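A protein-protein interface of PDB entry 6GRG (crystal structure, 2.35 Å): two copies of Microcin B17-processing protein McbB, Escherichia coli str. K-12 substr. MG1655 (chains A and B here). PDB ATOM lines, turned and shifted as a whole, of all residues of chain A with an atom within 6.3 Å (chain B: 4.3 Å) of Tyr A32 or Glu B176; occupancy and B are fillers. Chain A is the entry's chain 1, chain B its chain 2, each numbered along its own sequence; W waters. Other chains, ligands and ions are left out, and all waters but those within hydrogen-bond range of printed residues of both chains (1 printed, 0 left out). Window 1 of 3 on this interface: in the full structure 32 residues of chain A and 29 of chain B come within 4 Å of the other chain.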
ATOM      1  N   PRO A  17      -5.332 -11.655 -11.139  1.00  0.00           N
ATOM      2  CA  PRO A  17      -4.900 -10.576 -10.260  1.00  0.00           C
ATOM      3  C   PRO A  17      -5.757 -10.554  -8.988  1.00  0.00           C
ATOM      4  O   PRO A  17      -6.995 -10.535  -9.071  1.00  0.00           O
ATOM      5  CB  PRO A  17      -5.089  -9.290 -11.104  1.00  0.00           C
ATOM      6  CG  PRO A  17      -5.227  -9.773 -12.524  1.00  0.00           C
ATOM      7  CD  PRO A  17      -5.852 -11.154 -12.419  1.00  0.00           C
ATOM      8  N   PHE A  18      -5.090 -10.547  -7.831  1.00  0.00           N
ATOM      9  CA  PHE A  18      -5.769 -10.338  -6.562  1.00  0.00           C
ATOM     10  C   PHE A  18      -4.759  -9.928  -5.490  1.00  0.00           C
ATOM     11  O   PHE A  18      -3.570 -10.014  -5.685  1.00  0.00           O
ATOM     12  CB  PHE A  18      -6.504 -11.604  -6.133  1.00  0.00           C
ATOM     13  CG  PHE A  18      -5.597 -12.724  -5.702  1.00  0.00           C
ATOM     14  CD1 PHE A  18      -5.013 -13.565  -6.634  1.00  0.00           C
ATOM     15  CD2 PHE A  18      -5.342 -12.948  -4.356  1.00  0.00           C
ATOM     16  CE1 PHE A  18      -4.187 -14.600  -6.226  1.00  0.00           C
ATOM     17  CE2 PHE A  18      -4.515 -13.980  -3.952  1.00  0.00           C
ATOM     18  CZ  PHE A  18      -3.939 -14.800  -4.890  1.00  0.00           C
ATOM     19  N   ILE A  30      -9.356  -9.690  -2.243  1.00  0.00           N
ATOM     20  CA  ILE A  30      -9.922  -8.789  -3.226  1.00  0.00           C
ATOM     21  C   ILE A  30      -9.425  -9.194  -4.612  1.00  0.00           C
ATOM     22  O   ILE A  30      -8.258  -9.281  -4.843  1.00  0.00           O
ATOM     23  CB  ILE A  30      -9.553  -7.331  -2.927  1.00  0.00           C
ATOM     24  CG1 ILE A  30      -9.674  -7.010  -1.434  1.00  0.00           C
ATOM     25  CG2 ILE A  30     -10.400  -6.409  -3.789  1.00  0.00           C
ATOM     26  CD1 ILE A  30      -9.157  -5.643  -1.074  1.00  0.00           C
ATOM     27  N   THR A  31     -10.370  -9.398  -5.523  1.00  0.00           N
ATOM     28  CA  THR A  31     -10.103  -9.730  -6.899  1.00  0.00           C
ATOM     29  C   THR A  31     -10.896  -8.775  -7.788  1.00  0.00           C
ATOM     30  O   THR A  31     -11.622  -7.858  -7.310  1.00  0.00           O
ATOM     31  CB  THR A  31     -10.464 -11.196  -7.195  1.00  0.00           C
ATOM     32  OG1 THR A  31     -11.880 -11.356  -7.303  1.00  0.00           O
ATOM     33  CG2 THR A  31      -9.966 -12.155  -6.137  1.00  0.00           C
ATOM     34  N   TYR A  32     -10.765  -9.027  -9.091  1.00  0.00           N
ATOM     35  CA  TYR A  32     -11.461  -8.295 -10.112  1.00  0.00           C
ATOM     36  C   TYR A  32     -12.943  -8.634 -10.011  1.00  0.00           C
ATOM     37  O   TYR A  32     -13.759  -7.832 -10.398  1.00  0.00           O
ATOM     38  CB  TYR A  32     -10.857  -8.584 -11.494  1.00  0.00           C
ATOM     39  CG  TYR A  32      -9.586  -7.823 -11.809  1.00  0.00           C
ATOM     40  CD1 TYR A  32      -9.120  -6.808 -10.978  1.00  0.00           C
ATOM     41  CD2 TYR A  32      -8.863  -8.074 -12.966  1.00  0.00           C
ATOM     42  CE1 TYR A  32      -7.970  -6.086 -11.265  1.00  0.00           C
ATOM     43  CE2 TYR A  32      -7.713  -7.357 -13.273  1.00  0.00           C
ATOM     44  CZ  TYR A  32      -7.261  -6.370 -12.415  1.00  0.00           C
ATOM     45  OH  TYR A  32      -6.130  -5.660 -12.670  1.00  0.00           O
ATOM     46  N   ILE A  33     -13.247  -9.815  -9.459  1.00  0.00           N
ATOM     47  CA  ILE A  33     -14.584 -10.387  -9.458  1.00  0.00           C
ATOM     48  C   ILE A  33     -15.256 -10.066  -8.127  1.00  0.00           C
ATOM     49  O   ILE A  33     -16.462  -9.805  -8.074  1.00  0.00           O
ATOM     50  CB  ILE A  33     -14.525 -11.912  -9.722  1.00  0.00           C
ATOM     51  CG1 ILE A  33     -13.914 -12.229 -11.082  1.00  0.00           C
ATOM     52  CG2 ILE A  33     -15.891 -12.570  -9.607  1.00  0.00           C
ATOM     53  CD1 ILE A  33     -14.698 -11.648 -12.242  1.00  0.00           C
ATOM     54  N   SER A  34     -14.490 -10.124  -7.038  1.00  0.00           N
ATOM     55  CA  SER A  34     -15.128 -10.170  -5.762  1.00  0.00           C
ATOM     56  C   SER A  34     -14.159  -9.840  -4.616  1.00  0.00           C
ATOM     57  O   SER A  34     -12.939  -9.746  -4.783  1.00  0.00           O
ATOM     58  CB  SER A  34     -15.794 -11.527  -5.568  1.00  0.00           C
ATOM     59  OG  SER A  34     -14.845 -12.553  -5.277  1.00  0.00           O
ATOM     60  N   THR A  83     -14.767 -16.810  -6.934  1.00  0.00           N
ATOM     61  CA  THR A  83     -14.366 -15.559  -6.306  1.00  0.00           C
ATOM     62  C   THR A  83     -13.391 -14.758  -7.181  1.00  0.00           C
ATOM     63  O   THR A  83     -13.078 -13.644  -6.827  1.00  0.00           O
ATOM     64  CB  THR A  83     -13.708 -15.778  -4.937  1.00  0.00           C
ATOM     65  OG1 THR A  83     -12.542 -16.578  -5.132  1.00  0.00           O
ATOM     66  CG2 THR A  83     -14.609 -16.433  -3.914  1.00  0.00           C
ATOM     67  N   GLY A  84     -12.860 -15.349  -8.262  1.00  0.00           N
ATOM     68  CA  GLY A  84     -12.005 -14.665  -9.246  1.00  0.00           C
ATOM     69  C   GLY A  84     -10.508 -14.761  -8.962  1.00  0.00           C
ATOM     70  O   GLY A  84      -9.707 -13.908  -9.440  1.00  0.00           O
ATOM     71  N   ARG A 248      -0.010  -6.260 -22.870  1.00  0.00           N
ATOM     72  CA  ARG A 248      -1.464  -6.494 -22.856  1.00  0.00           C
ATOM     73  C   ARG A 248      -1.918  -7.077 -24.190  1.00  0.00           C
ATOM     74  O   ARG A 248      -2.778  -7.943 -24.221  1.00  0.00           O
ATOM     75  CB  ARG A 248      -2.248  -5.223 -22.526  1.00  0.00           C
ATOM     76  CG  ARG A 248      -2.225  -4.866 -21.049  1.00  0.00           C
ATOM     77  CD  ARG A 248      -2.799  -5.944 -20.144  1.00  0.00           C
ATOM     78  NE  ARG A 248      -3.057  -5.401 -18.818  1.00  0.00           N
ATOM     79  CZ  ARG A 248      -2.948  -6.091 -17.696  1.00  0.00           C
ATOM     80  NH1 ARG A 248      -2.544  -7.350 -17.743  1.00  0.00           N
ATOM     81  NH2 ARG A 248      -3.233  -5.521 -16.536  1.00  0.00           N
ATOM     82  N   LEU A 258      -8.119 -11.807 -19.464  1.00  0.00           N
ATOM     83  CA  LEU A 258      -8.906 -11.222 -18.398  1.00  0.00           C
ATOM     84  C   LEU A 258     -10.248 -10.727 -18.962  1.00  0.00           C
ATOM     85  O   LEU A 258     -11.288 -10.907 -18.352  1.00  0.00           O
ATOM     86  CB  LEU A 258      -8.071 -10.107 -17.757  1.00  0.00           C
ATOM     87  CG  LEU A 258      -6.828 -10.581 -16.995  1.00  0.00           C
ATOM     88  CD1 LEU A 258      -5.981  -9.421 -16.476  1.00  0.00           C
ATOM     89  CD2 LEU A 258      -7.222 -11.485 -15.848  1.00  0.00           C
ATOM     90  N   LEU B 174      -8.614   1.522  -8.205  1.00  0.00           N
ATOM     91  CA  LEU B 174      -9.888   0.913  -7.852  1.00  0.00           C
ATOM     92  C   LEU B 174     -10.094  -0.296  -8.761  1.00  0.00           C
ATOM     93  O   LEU B 174     -10.520  -0.123  -9.901  1.00  0.00           O
ATOM     94  CB  LEU B 174     -11.030   1.909  -8.083  1.00  0.00           C
ATOM     95  CG  LEU B 174     -10.964   3.239  -7.332  1.00  0.00           C
ATOM     96  CD1 LEU B 174     -11.816   4.304  -8.038  1.00  0.00           C
ATOM     97  CD2 LEU B 174     -11.391   3.063  -5.876  1.00  0.00           C
ATOM     98  N   LYS B 175      -9.805  -1.496  -8.240  1.00  0.00           N
ATOM     99  CA  LYS B 175      -9.908  -2.770  -8.982  1.00  0.00           C
ATOM    100  C   LYS B 175      -9.011  -2.654 -10.227  1.00  0.00           C
ATOM    101  O   LYS B 175      -7.804  -2.484 -10.062  1.00  0.00           O
ATOM    102  CB  LYS B 175     -11.369  -3.131  -9.290  1.00  0.00           C
ATOM    103  CG  LYS B 175     -12.037  -4.057  -8.288  1.00  0.00           C
ATOM    104  CD  LYS B 175     -13.071  -4.987  -8.889  1.00  0.00           C
ATOM    105  CE  LYS B 175     -14.251  -4.268  -9.511  1.00  0.00           C
ATOM    106  NZ  LYS B 175     -14.481  -4.726 -10.908  1.00  0.00           N
ATOM    107  N   GLU B 176      -9.591  -2.683 -11.440  1.00  0.00           N
ATOM    108  CA  GLU B 176      -8.794  -2.718 -12.671  1.00  0.00           C
ATOM    109  C   GLU B 176      -8.506  -1.285 -13.157  1.00  0.00           C
ATOM    110  O   GLU B 176      -7.785  -1.114 -14.120  1.00  0.00           O
ATOM    111  CB  GLU B 176      -9.449  -3.581 -13.754  1.00  0.00           C
ATOM    112  CG  GLU B 176     -10.753  -3.034 -14.282  1.00  0.00           C
ATOM    113  CD  GLU B 176     -11.887  -3.040 -13.270  1.00  0.00           C
ATOM    114  OE1 GLU B 176     -11.828  -3.858 -12.341  1.00  0.00           O
ATOM    115  OE2 GLU B 176     -12.812  -2.212 -13.404  1.00  0.00           O
ATOM    116  N   SER B 177      -9.013  -0.263 -12.455  1.00  0.00           N
ATOM    117  CA  SER B 177      -8.966   1.072 -12.953  1.00  0.00           C
ATOM    118  C   SER B 177      -7.875   1.869 -12.242  1.00  0.00           C
ATOM    119  O   SER B 177      -7.680   1.728 -11.024  1.00  0.00           O
ATOM    120  CB  SER B 177     -10.286   1.757 -12.812  1.00  0.00           C
ATOM    121  OG  SER B 177     -11.197   1.245 -13.762  1.00  0.00           O
ATOM    122  N   PHE B 178      -7.182   2.705 -13.030  1.00  0.00           N
ATOM    123  CA  PHE B 178      -6.378   3.812 -12.521  1.00  0.00           C
ATOM    124  C   PHE B 178      -7.228   5.086 -12.631  1.00  0.00           C
ATOM    125  O   PHE B 178      -7.670   5.424 -13.728  1.00  0.00           O
ATOM    126  CB  PHE B 178      -5.066   3.873 -13.294  1.00  0.00           C
ATOM    127  CG  PHE B 178      -4.144   4.970 -12.856  1.00  0.00           C
ATOM    128  CD1 PHE B 178      -3.838   5.137 -11.520  1.00  0.00           C
ATOM    129  CD2 PHE B 178      -3.587   5.838 -13.779  1.00  0.00           C
ATOM    130  CE1 PHE B 178      -2.969   6.130 -11.114  1.00  0.00           C
ATOM    131  CE2 PHE B 178      -2.751   6.861 -13.366  1.00  0.00           C
ATOM    132  CZ  PHE B 178      -2.445   7.008 -12.034  1.00  0.00           C
ATOM    133  N   LEU B 232      -4.449  -3.768  -7.167  1.00  0.00           N
ATOM    134  CA  LEU B 232      -4.457  -5.189  -7.331  1.00  0.00           C
ATOM    135  C   LEU B 232      -3.304  -5.621  -8.250  1.00  0.00           C
ATOM    136  O   LEU B 232      -3.404  -5.533  -9.487  1.00  0.00           O
ATOM    137  CB  LEU B 232      -5.818  -5.603  -7.896  1.00  0.00           C
ATOM    138  CG  LEU B 232      -6.754  -6.261  -6.892  1.00  0.00           C
ATOM    139  CD1 LEU B 232      -6.874  -5.419  -5.626  1.00  0.00           C
ATOM    140  CD2 LEU B 232      -8.105  -6.507  -7.537  1.00  0.00           C
ATOM    141  N   ALA B 272      -8.547   4.994 -16.409  1.00  0.00           N
ATOM    142  CA  ALA B 272      -7.876   4.109 -17.390  1.00  0.00           C
ATOM    143  C   ALA B 272      -8.054   2.647 -16.955  1.00  0.00           C
ATOM    144  O   ALA B 272      -7.629   2.255 -15.866  1.00  0.00           O
ATOM    145  CB  ALA B 272      -6.410   4.467 -17.493  1.00  0.00           C
ATOM    146  N   ASP B 273      -8.707   1.858 -17.805  1.00  0.00           N
ATOM    147  CA  ASP B 273      -8.854   0.440 -17.597  1.00  0.00           C
ATOM    148  C   ASP B 273      -7.484  -0.186 -17.874  1.00  0.00           C
ATOM    149  O   ASP B 273      -6.993  -0.103 -18.959  1.00  0.00           O
ATOM    150  CB  ASP B 273      -9.979  -0.122 -18.470  1.00  0.00           C
ATOM    151  CG  ASP B 273     -10.178  -1.623 -18.348  1.00  0.00           C
ATOM    152  OD1 ASP B 273      -9.198  -2.343 -18.034  1.00  0.00           O
ATOM    153  OD2 ASP B 273     -11.311  -2.066 -18.577  1.00  0.00           O
ATOM    154  N   LEU B 274      -6.838  -0.734 -16.846  1.00  0.00           N
ATOM    155  CA  LEU B 274      -5.458  -1.194 -16.963  1.00  0.00           C
ATOM    156  C   LEU B 274      -5.365  -2.483 -17.799  1.00  0.00           C
ATOM    157  O   LEU B 274      -4.279  -2.910 -18.177  1.00  0.00           O
ATOM    158  CB  LEU B 274      -4.907  -1.421 -15.557  1.00  0.00           C
ATOM    159  CG  LEU B 274      -4.578  -0.167 -14.764  1.00  0.00           C
ATOM    160  CD1 LEU B 274      -3.958  -0.522 -13.413  1.00  0.00           C
ATOM    161  CD2 LEU B 274      -3.647   0.720 -15.560  1.00  0.00           C
ATOM    162  N   ILE B 275      -6.493  -3.134 -18.049  1.00  0.00           N
ATOM    163  CA  ILE B 275      -6.479  -4.339 -18.815  1.00  0.00           C
ATOM    164  C   ILE B 275      -6.536  -3.955 -20.299  1.00  0.00           C
ATOM    165  O   ILE B 275      -5.589  -4.225 -21.031  1.00  0.00           O
ATOM    166  CB  ILE B 275      -7.635  -5.288 -18.422  1.00  0.00           C
ATOM    167  CG1 ILE B 275      -7.727  -5.518 -16.909  1.00  0.00           C
ATOM    168  CG2 ILE B 275      -7.504  -6.602 -19.188  1.00  0.00           C
ATOM    169  CD1 ILE B 275      -9.019  -6.194 -16.446  1.00  0.00           C
HETATM  170  O   HOH W   1      -4.994  -3.635 -10.788  1.00  0.00           O
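NE of Arg A248 is in hydrogen-bond range of O of Leu B274.
The backbone carbonyl oxygen (O) of Tyr A32 lies within hydrogen-bond range of the side-chain amino group (NZ) of Lys B175, 3.2 Å away.
Hydrophobic or aromatic side chains of chain B that line the printed part of chain A: Leu B232 and Ile B275.
Hydrophobic or aromatic side chains of chain A within 4 Å of the printed part of chain B: Tyr A32 and Leu A258.
Among the printed residues, no Asp or Glu carboxylate lies within 4 Å of a Lys or Arg side-chain nitrogen of the other chain.
O of Thr A83 is in hydrogen-bond range of OG1 of Thr A31 (2.6 Å).
The side-chain amino group (NZ) of Lys B175 is in salt-bridge range of the side-chain carboxylate (OE1) of Glu B176, 3.1 Å away.
OG1 of Thr A31 lies within hydrogen-bond range of N of Ser A34.
The backbone NH (N) of Ile B275 is in hydrogen-bond range of the side-chain carboxylate (OD1) of Asp B273 (2.8 Å).
The backbone NH (N) of Ile A33 is in hydrogen-bond range of the side-chain hydroxyl (OG1) of Thr A31, at 3.0 Å.
The backbone NH (N) of Leu B274 lies within hydrogen-bond range of the backbone carbonyl oxygen (O) of Glu B176, 2.9 Å away.
Water W1 lies within hydrogen-bond range of O of Leu B232 (2.8 Å), OH of Tyr A32 (3.0 Å) and O of Lys B175 (3.1 Å).
Among the printed residues, pairs that only touch across the chains: Arg A248 with Ile B275, Thr A31 with Lys B175, Tyr A32 with Leu B232, Thr A31 with Leu B232, Tyr A32 with Ile B275, Tyr A32 with Glu B176, Leu A258 with Ile B275 and Ile A30 with Leu B232.
No position is printed for both chains.
Of the printed residues of chain B, Ile A30 touches Leu B232 (3.9 Å).
Tyr A32 touches just these residues of chain B: Lys B175 (3.2 Å), Glu B176 (3.7 Å), Leu B232 (3.6 Å) and Ile B275 (3.6 Å).
Gly A84 touches none of the printed residues of chain B.
Printed residues of chain B within 4 Å of Arg A248: Leu B274 (2.8 Å) and Ile B275 (3.4 Å).
Of the printed residues of chain A, Lys B175 touches Thr A31 (3.6 Å) and Tyr A32 (3.2 Å).
Glu B176 touches just one residue of chain A: Tyr A32.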
